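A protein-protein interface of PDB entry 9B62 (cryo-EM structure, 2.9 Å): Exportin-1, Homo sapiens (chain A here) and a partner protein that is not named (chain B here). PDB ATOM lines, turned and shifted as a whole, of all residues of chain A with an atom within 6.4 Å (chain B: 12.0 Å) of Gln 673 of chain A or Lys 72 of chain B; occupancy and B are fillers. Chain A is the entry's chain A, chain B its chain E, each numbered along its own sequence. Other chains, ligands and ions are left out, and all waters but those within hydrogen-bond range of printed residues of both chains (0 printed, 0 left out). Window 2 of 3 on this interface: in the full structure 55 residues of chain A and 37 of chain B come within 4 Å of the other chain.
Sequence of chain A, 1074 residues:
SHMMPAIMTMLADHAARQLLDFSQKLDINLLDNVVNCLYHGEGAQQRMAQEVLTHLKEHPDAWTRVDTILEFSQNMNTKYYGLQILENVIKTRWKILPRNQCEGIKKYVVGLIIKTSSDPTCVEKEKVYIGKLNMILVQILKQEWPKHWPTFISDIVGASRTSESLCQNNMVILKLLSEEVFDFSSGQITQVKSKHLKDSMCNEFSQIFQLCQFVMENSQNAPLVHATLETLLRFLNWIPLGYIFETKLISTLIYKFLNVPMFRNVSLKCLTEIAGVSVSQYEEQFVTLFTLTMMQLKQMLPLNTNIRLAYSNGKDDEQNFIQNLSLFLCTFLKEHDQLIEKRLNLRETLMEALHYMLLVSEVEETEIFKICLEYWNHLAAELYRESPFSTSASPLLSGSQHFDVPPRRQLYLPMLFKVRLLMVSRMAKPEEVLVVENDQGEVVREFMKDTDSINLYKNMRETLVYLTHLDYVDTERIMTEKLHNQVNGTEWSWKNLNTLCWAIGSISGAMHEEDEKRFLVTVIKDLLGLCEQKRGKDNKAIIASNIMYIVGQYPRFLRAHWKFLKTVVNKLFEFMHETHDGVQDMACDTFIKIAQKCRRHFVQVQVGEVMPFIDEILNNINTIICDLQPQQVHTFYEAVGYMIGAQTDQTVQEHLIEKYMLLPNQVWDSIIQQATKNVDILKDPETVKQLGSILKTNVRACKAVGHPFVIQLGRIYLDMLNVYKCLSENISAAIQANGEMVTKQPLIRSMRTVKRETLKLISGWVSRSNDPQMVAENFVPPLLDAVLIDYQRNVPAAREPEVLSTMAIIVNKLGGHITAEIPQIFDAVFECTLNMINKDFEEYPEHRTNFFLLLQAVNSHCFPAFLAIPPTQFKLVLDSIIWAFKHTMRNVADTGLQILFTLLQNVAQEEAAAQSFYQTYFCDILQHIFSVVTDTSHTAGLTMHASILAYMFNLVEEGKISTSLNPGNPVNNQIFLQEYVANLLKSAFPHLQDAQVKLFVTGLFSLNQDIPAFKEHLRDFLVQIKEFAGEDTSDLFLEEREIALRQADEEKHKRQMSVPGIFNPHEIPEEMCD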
ATOM      1  N   TRP A 668       5.418  28.687  19.181  1.00  0.00           N
ATOM      2  CA  TRP A 668       4.608  28.101  18.122  1.00  0.00           C
ATOM      3  C   TRP A 668       4.894  28.758  16.780  1.00  0.00           C
ATOM      4  O   TRP A 668       5.028  28.072  15.762  1.00  0.00           O
ATOM      5  CB  TRP A 668       3.128  28.232  18.481  1.00  0.00           C
ATOM      6  CG  TRP A 668       2.196  27.739  17.427  1.00  0.00           C
ATOM      7  CD1 TRP A 668       1.650  28.467  16.413  1.00  0.00           C
ATOM      8  CD2 TRP A 668       1.687  26.410  17.287  1.00  0.00           C
ATOM      9  NE1 TRP A 668       0.836  27.672  15.646  1.00  0.00           N
ATOM     10  CE2 TRP A 668       0.844  26.403  16.163  1.00  0.00           C
ATOM     11  CE3 TRP A 668       1.868  25.224  18.001  1.00  0.00           C
ATOM     12  CZ2 TRP A 668       0.180  25.258  15.738  1.00  0.00           C
ATOM     13  CZ3 TRP A 668       1.209  24.089  17.577  1.00  0.00           C
ATOM     14  CH2 TRP A 668       0.377  24.114  16.456  1.00  0.00           C
ATOM     15  N   ASP A 669       4.974  30.088  16.754  1.00  0.00           N
ATOM     16  CA  ASP A 669       5.276  30.789  15.514  1.00  0.00           C
ATOM     17  C   ASP A 669       6.660  30.427  15.010  1.00  0.00           C
ATOM     18  O   ASP A 669       6.860  30.251  13.806  1.00  0.00           O
ATOM     19  CB  ASP A 669       5.161  32.297  15.722  1.00  0.00           C
ATOM     20  CG  ASP A 669       3.749  32.735  16.043  1.00  0.00           C
ATOM     21  OD1 ASP A 669       2.838  31.883  16.009  1.00  0.00           O
ATOM     22  OD2 ASP A 669       3.548  33.934  16.331  1.00  0.00           O
ATOM     23  N   SER A 670       7.636  30.318  15.913  1.00  0.00           N
ATOM     24  CA  SER A 670       8.971  29.903  15.495  1.00  0.00           C
ATOM     25  C   SER A 670       8.925  28.538  14.823  1.00  0.00           C
ATOM     26  O   SER A 670       9.475  28.349  13.730  1.00  0.00           O
ATOM     27  CB  SER A 670       9.909  29.879  16.699  1.00  0.00           C
ATOM     28  OG  SER A 670      11.187  29.390  16.337  1.00  0.00           O
ATOM     29  N   ILE A 671       8.250  27.575  15.455  1.00  0.00           N
ATOM     30  CA  ILE A 671       8.202  26.222  14.902  1.00  0.00           C
ATOM     31  C   ILE A 671       7.476  26.214  13.563  1.00  0.00           C
ATOM     32  O   ILE A 671       7.899  25.540  12.618  1.00  0.00           O
ATOM     33  CB  ILE A 671       7.550  25.254  15.905  1.00  0.00           C
ATOM     34  CG1 ILE A 671       8.470  25.043  17.107  1.00  0.00           C
ATOM     35  CG2 ILE A 671       7.242  23.928  15.229  1.00  0.00           C
ATOM     36  CD1 ILE A 671       7.836  24.272  18.239  1.00  0.00           C
ATOM     37  N   ILE A 672       6.362  26.942  13.462  1.00  0.00           N
ATOM     38  CA  ILE A 672       5.584  26.935  12.225  1.00  0.00           C
ATOM     39  C   ILE A 672       6.361  27.598  11.097  1.00  0.00           C
ATOM     40  O   ILE A 672       6.350  27.122   9.955  1.00  0.00           O
ATOM     41  CB  ILE A 672       4.221  27.614  12.449  1.00  0.00           C
ATOM     42  CG1 ILE A 672       3.351  26.782  13.395  1.00  0.00           C
ATOM     43  CG2 ILE A 672       3.513  27.831  11.127  1.00  0.00           C
ATOM     44  CD1 ILE A 672       3.018  25.393  12.892  1.00  0.00           C
ATOM     45  N   GLN A 673       7.036  28.711  11.386  1.00  0.00           N
ATOM     46  CA  GLN A 673       7.852  29.362  10.369  1.00  0.00           C
ATOM     47  C   GLN A 673       8.984  28.450   9.921  1.00  0.00           C
ATOM     48  O   GLN A 673       9.319  28.399   8.733  1.00  0.00           O
ATOM     49  CB  GLN A 673       8.408  30.678  10.914  1.00  0.00           C
ATOM     50  CG  GLN A 673       8.938  31.620   9.850  1.00  0.00           C
ATOM     51  CD  GLN A 673       7.832  32.232   9.016  1.00  0.00           C
ATOM     52  OE1 GLN A 673       6.652  31.965   9.238  1.00  0.00           O
ATOM     53  NE2 GLN A 673       8.209  33.060   8.050  1.00  0.00           N
ATOM     54  N   GLN A 674       9.590  27.726  10.863  1.00  0.00           N
ATOM     55  CA  GLN A 674      10.639  26.781  10.503  1.00  0.00           C
ATOM     56  C   GLN A 674      10.094  25.667   9.617  1.00  0.00           C
ATOM     57  O   GLN A 674      10.732  25.278   8.632  1.00  0.00           O
ATOM     58  CB  GLN A 674      11.262  26.207  11.773  1.00  0.00           C
ATOM     59  CG  GLN A 674      12.632  25.598  11.587  1.00  0.00           C
ATOM     60  CD  GLN A 674      13.315  25.323  12.907  1.00  0.00           C
ATOM     61  OE1 GLN A 674      12.693  25.395  13.967  1.00  0.00           O
ATOM     62  NE2 GLN A 674      14.605  25.012  12.855  1.00  0.00           N
ATOM     63  N   ALA A 675       8.912  25.144   9.951  1.00  0.00           N
ATOM     64  CA  ALA A 675       8.323  24.062   9.169  1.00  0.00           C
ATOM     65  C   ALA A 675       7.924  24.526   7.777  1.00  0.00           C
ATOM     66  O   ALA A 675       7.982  23.741   6.825  1.00  0.00           O
ATOM     67  CB  ALA A 675       7.107  23.489   9.895  1.00  0.00           C
ATOM     68  N   THR A 676       7.509  25.785   7.637  1.00  0.00           N
ATOM     69  CA  THR A 676       7.147  26.293   6.319  1.00  0.00           C
ATOM     70  C   THR A 676       8.299  26.133   5.335  1.00  0.00           C
ATOM     71  O   THR A 676       8.081  25.835   4.154  1.00  0.00           O
ATOM     72  CB  THR A 676       6.729  27.761   6.417  1.00  0.00           C
ATOM     73  OG1 THR A 676       5.577  27.876   7.261  1.00  0.00           O
ATOM     74  CG2 THR A 676       6.402  28.320   5.044  1.00  0.00           C
ATOM     75  N   LYS A 677       9.535  26.329   5.799  1.00  0.00           N
ATOM     76  CA  LYS A 677      10.689  26.133   4.928  1.00  0.00           C
ATOM     77  C   LYS A 677      10.798  24.680   4.482  1.00  0.00           C
ATOM     78  O   LYS A 677      11.061  24.400   3.307  1.00  0.00           O
ATOM     79  CB  LYS A 677      11.967  26.566   5.645  1.00  0.00           C
ATOM     80  CG  LYS A 677      11.934  27.985   6.187  1.00  0.00           C
ATOM     81  CD  LYS A 677      11.769  29.009   5.079  1.00  0.00           C
ATOM     82  CE  LYS A 677      11.807  30.428   5.624  1.00  0.00           C
ATOM     83  NZ  LYS A 677      13.119  30.759   6.244  1.00  0.00           N
ATOM     84  N   ASN A 678      10.602  23.742   5.407  1.00  0.00           N
ATOM     85  CA  ASN A 678      10.639  22.322   5.085  1.00  0.00           C
ATOM     86  C   ASN A 678       9.883  21.566   6.166  1.00  0.00           C
ATOM     87  O   ASN A 678      10.131  21.776   7.357  1.00  0.00           O
ATOM     88  CB  ASN A 678      12.080  21.812   4.982  1.00  0.00           C
ATOM     89  CG  ASN A 678      12.825  21.906   6.295  1.00  0.00           C
ATOM     90  OD1 ASN A 678      12.570  22.798   7.103  1.00  0.00           O
ATOM     91  ND2 ASN A 678      13.750  20.982   6.517  1.00  0.00           N
ATOM     92  N   ILE A 681      11.197  18.990   9.445  1.00  0.00           N
ATOM     93  CA  ILE A 681      11.581  19.243  10.829  1.00  0.00           C
ATOM     94  C   ILE A 681      10.614  18.565  11.787  1.00  0.00           C
ATOM     95  O   ILE A 681      11.012  18.125  12.872  1.00  0.00           O
ATOM     96  CB  ILE A 681      11.675  20.755  11.101  1.00  0.00           C
ATOM     97  CG1 ILE A 681      10.287  21.395  11.142  1.00  0.00           C
ATOM     98  CG2 ILE A 681      12.534  21.427  10.042  1.00  0.00           C
ATOM     99  CD1 ILE A 681      10.319  22.857  11.495  1.00  0.00           C
ATOM    100  N   LEU A 718      -5.754  26.753  12.108  1.00  0.00           N
ATOM    101  CA  LEU A 718      -5.434  26.105  10.840  1.00  0.00           C
ATOM    102  C   LEU A 718      -4.022  25.534  10.848  1.00  0.00           C
ATOM    103  O   LEU A 718      -3.778  24.460  10.283  1.00  0.00           O
ATOM    104  CB  LEU A 718      -5.618  27.089   9.687  1.00  0.00           C
ATOM    105  CG  LEU A 718      -7.026  27.676   9.547  1.00  0.00           C
ATOM    106  CD1 LEU A 718      -7.128  28.526   8.300  1.00  0.00           C
ATOM    107  CD2 LEU A 718      -8.080  26.584   9.528  1.00  0.00           C
ATOM    108  N   ASP A 719      -3.079  26.229  11.481  1.00  0.00           N
ATOM    109  CA  ASP A 719      -1.740  25.671  11.631  1.00  0.00           C
ATOM    110  C   ASP A 719      -1.774  24.399  12.467  1.00  0.00           C
ATOM    111  O   ASP A 719      -1.080  23.421  12.156  1.00  0.00           O
ATOM    112  CB  ASP A 719      -0.812  26.706  12.262  1.00  0.00           C
ATOM    113  CG  ASP A 719      -0.658  27.945  11.406  1.00  0.00           C
ATOM    114  OD1 ASP A 719      -0.644  27.811  10.166  1.00  0.00           O
ATOM    115  OD2 ASP A 719      -0.554  29.053  11.972  1.00  0.00           O
ATOM    116  N   ASN A 722      -3.051  21.636  10.240  1.00  0.00           N
ATOM    117  CA  ASN A 722      -2.056  21.200   9.263  1.00  0.00           C
ATOM    118  C   ASN A 722      -0.982  20.334   9.909  1.00  0.00           C
ATOM    119  O   ASN A 722      -0.579  19.309   9.343  1.00  0.00           O
ATOM    120  CB  ASN A 722      -1.428  22.412   8.579  1.00  0.00           C
ATOM    121  CG  ASN A 722      -2.402  23.141   7.680  1.00  0.00           C
ATOM    122  OD1 ASN A 722      -3.304  22.536   7.104  1.00  0.00           O
ATOM    123  ND2 ASN A 722      -2.226  24.449   7.555  1.00  0.00           N
ATOM    124  N   VAL B  68     -10.995  33.085  12.060  1.00  0.00           N
ATOM    125  CA  VAL B  68      -9.946  32.088  11.878  1.00  0.00           C
ATOM    126  C   VAL B  68      -8.908  32.673  10.931  1.00  0.00           C
ATOM    127  O   VAL B  68      -9.223  32.995   9.779  1.00  0.00           O
ATOM    128  CB  VAL B  68     -10.503  30.765  11.332  1.00  0.00           C
ATOM    129  CG1 VAL B  68      -9.390  29.748  11.170  1.00  0.00           C
ATOM    130  CG2 VAL B  68     -11.583  30.226  12.249  1.00  0.00           C
ATOM    131  N   SER B  69      -7.677  32.808  11.413  1.00  0.00           N
ATOM    132  CA  SER B  69      -6.617  33.373  10.598  1.00  0.00           C
ATOM    133  C   SER B  69      -6.172  32.372   9.533  1.00  0.00           C
ATOM    134  O   SER B  69      -6.296  31.159   9.719  1.00  0.00           O
ATOM    135  CB  SER B  69      -5.428  33.765  11.469  1.00  0.00           C
ATOM    136  OG  SER B  69      -5.783  34.784  12.386  1.00  0.00           O
ATOM    137  N   PRO B  70      -5.644  32.852   8.410  1.00  0.00           N
ATOM    138  CA  PRO B  70      -5.188  31.940   7.355  1.00  0.00           C
ATOM    139  C   PRO B  70      -3.984  31.137   7.810  1.00  0.00           C
ATOM    140  O   PRO B  70      -3.280  31.536   8.750  1.00  0.00           O
ATOM    141  CB  PRO B  70      -4.828  32.887   6.201  1.00  0.00           C
ATOM    142  CG  PRO B  70      -4.524  34.180   6.860  1.00  0.00           C
ATOM    143  CD  PRO B  70      -5.440  34.262   8.040  1.00  0.00           C
ATOM    144  N   PRO B  71      -3.716  29.994   7.175  1.00  0.00           N
ATOM    145  CA  PRO B  71      -2.612  29.129   7.618  1.00  0.00           C
ATOM    146  C   PRO B  71      -1.282  29.589   7.039  1.00  0.00           C
ATOM    147  O   PRO B  71      -1.115  29.656   5.820  1.00  0.00           O
ATOM    148  CB  PRO B  71      -3.013  27.752   7.080  1.00  0.00           C
ATOM    149  CG  PRO B  71      -3.764  28.069   5.828  1.00  0.00           C
ATOM    150  CD  PRO B  71      -4.458  29.396   6.050  1.00  0.00           C
ATOM    151  N   LYS B  72      -0.334  29.913   7.920  1.00  0.00           N
ATOM    152  CA  LYS B  72       1.028  30.175   7.467  1.00  0.00           C
ATOM    153  C   LYS B  72       1.660  28.917   6.886  1.00  0.00           C
ATOM    154  O   LYS B  72       2.353  28.977   5.863  1.00  0.00           O
ATOM    155  CB  LYS B  72       1.875  30.708   8.621  1.00  0.00           C
ATOM    156  CG  LYS B  72       1.576  32.147   9.007  1.00  0.00           C
ATOM    157  CD  LYS B  72       2.230  32.518  10.332  1.00  0.00           C
ATOM    158  CE  LYS B  72       3.744  32.354  10.291  1.00  0.00           C
ATOM    159  NZ  LYS B  72       4.384  32.743  11.578  1.00  0.00           N
ATOM    160  N   PHE B  73       1.431  27.772   7.525  1.00  0.00           N
ATOM    161  CA  PHE B  73       1.985  26.488   7.108  1.00  0.00           C
ATOM    162  C   PHE B  73       0.853  25.647   6.533  1.00  0.00           C
ATOM    163  O   PHE B  73      -0.062  25.247   7.259  1.00  0.00           O
ATOM    164  CB  PHE B  73       2.655  25.788   8.288  1.00  0.00           C
ATOM    165  CG  PHE B  73       2.886  24.319   8.077  1.00  0.00           C
ATOM    166  CD1 PHE B  73       3.608  23.865   6.988  1.00  0.00           C
ATOM    167  CD2 PHE B  73       2.399  23.395   8.982  1.00  0.00           C
ATOM    168  CE1 PHE B  73       3.825  22.517   6.799  1.00  0.00           C
ATOM    169  CE2 PHE B  73       2.616  22.047   8.797  1.00  0.00           C
ATOM    170  CZ  PHE B  73       3.329  21.608   7.705  1.00  0.00           C
ATOM    171  N   VAL B  74       0.917  25.381   5.231  1.00  0.00           N
ATOM    172  CA  VAL B  74      -0.099  24.608   4.524  1.00  0.00           C
ATOM    173  C   VAL B  74       0.529  23.288   4.102  1.00  0.00           C
ATOM    174  O   VAL B  74       1.537  23.272   3.385  1.00  0.00           O
ATOM    175  CB  VAL B  74      -0.647  25.370   3.308  1.00  0.00           C
ATOM    176  CG1 VAL B  74      -1.849  24.644   2.725  1.00  0.00           C
ATOM    177  CG2 VAL B  74      -1.010  26.790   3.697  1.00  0.00           C
ATOM    178  N   PHE B  75      -0.069  22.184   4.540  1.00  0.00           N
ATOM    179  CA  PHE B  75       0.429  20.846   4.247  1.00  0.00           C
ATOM    180  C   PHE B  75      -0.375  20.272   3.087  1.00  0.00           C
ATOM    181  O   PHE B  75      -1.557  19.944   3.244  1.00  0.00           O
ATOM    182  CB  PHE B  75       0.333  19.951   5.479  1.00  0.00           C
ATOM    183  CG  PHE B  75       0.882  18.572   5.268  1.00  0.00           C
ATOM    184  CD1 PHE B  75       2.232  18.318   5.429  1.00  0.00           C
ATOM    185  CD2 PHE B  75       0.048  17.529   4.909  1.00  0.00           C
ATOM    186  CE1 PHE B  75       2.741  17.050   5.235  1.00  0.00           C
ATOM    187  CE2 PHE B  75       0.551  16.258   4.713  1.00  0.00           C
ATOM    188  CZ  PHE B  75       1.899  16.018   4.877  1.00  0.00           C
ATOM    189  N   GLY B  76       0.263  20.148   1.929  1.00  0.00           N
ATOM    190  CA  GLY B  76      -0.391  19.604   0.754  1.00  0.00           C
ATOM    191  C   GLY B  76      -0.786  18.152   0.931  1.00  0.00           C
ATOM    192  O   GLY B  76       0.052  17.301   1.230  1.00  0.00           O
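Among the printed residues, pairs that only touch across the chains: Leu 718 of chain A with Ser 69 of chain B (3.1 Å), Asn 722 of chain A with Pro 71 of chain B (3.4 Å), Asp 719 of chain A with Pro 71 of chain B (3.5 Å), Leu 718 of chain A with Val 68 of chain B (3.5 Å), Leu 718 of chain A with Pro 71 of chain B (3.6 Å), Ile 672 of chain A with Phe 73 of chain B (3.6 Å), Thr 676 of chain A with Lys 72 of chain B (3.7 Å), Asn 722 of chain A with Val 74 of chain B (3.7 Å) and Thr 676 of chain A with Phe 73 of chain B (3.7 Å).
Asp 669 of chain A touches none of the printed residues of chain B.
No residue of chain B comes within 4 Å of Ser 670 of chain A.
Of chain B, only Phe 73 comes within 4 Å of Ile 672 of chain A.
Of chain B, only Lys 72 comes within 4 Å of Gln 673 of chain A.
No residue of chain B comes within 4 Å of Ala 675 of chain A.
Thr 676 of chain A touches just these residues of chain B: Lys 72 (3.7 Å) and Phe 73 (3.7 Å).
No residue of chain B comes within 4 Å of Lys 677 of chain A.
Of the printed residues of chain B, Leu 718 of chain A touches Val 68, Ser 69 and Pro 71.
Of the printed residues of chain A, Val 68 of chain B touches Leu 718 (3.5 Å).
Of the printed residues of chain A, Lys 72 of chain B touches Gln 673 (3.1 Å), Thr 676 (3.7 Å) and Asp 719 (3.1 Å).
Printed residues of chain A within 4 Å of Phe 73 of chain B: Ile 672 (3.6 Å), Thr 676 (3.7 Å), Asp 719 (3.4 Å) and Asn 722 (2.3 Å).
Hydrophobic or aromatic side chains of chain B within 4 Å of the printed part of chain A: Val 68, Pro 71 and Phe 73.
Hydrophobic or aromatic side chains of chain A that line the printed part of chain B: Ile 672 and Leu 718.
Among the printed residues, 13 pairs touch across the chains.
Among the printed residues, no Asp or Glu carboxylate lies within 4 Å of a Lys or Arg side-chain nitrogen of the other chain.
The side-chain amide oxygen (OE1) of Gln 673 of chain A sits close to the side-chain amino group (NZ) of Lys 72 of chain B.
The side-chain carboxylate of Asp 719 of chain A sits at hydrogen-bond distance from the backbone NH of Phe 73 of chain B (3.4 Å).
OD1 of Asp 719 of chain A lies within hydrogen-bond range of N of Lys 72 of chain B (3.1 Å).
The side-chain amide nitrogen (ND2) of Asn 722 of chain A lies close to the backbone carbonyl oxygen (O) of Phe 73 of chain B (2.3 Å).
The side-chain hydroxyl of Thr 676 of chain A lies within hydrogen-bond range of the backbone carbonyl oxygen of Ile 672 of chain A (2.9 Å).
The side-chain amide nitrogen of Asn 722 of chain A sits at hydrogen-bond distance from the backbone carbonyl oxygen of Leu 718 of chain A (3.1 Å).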
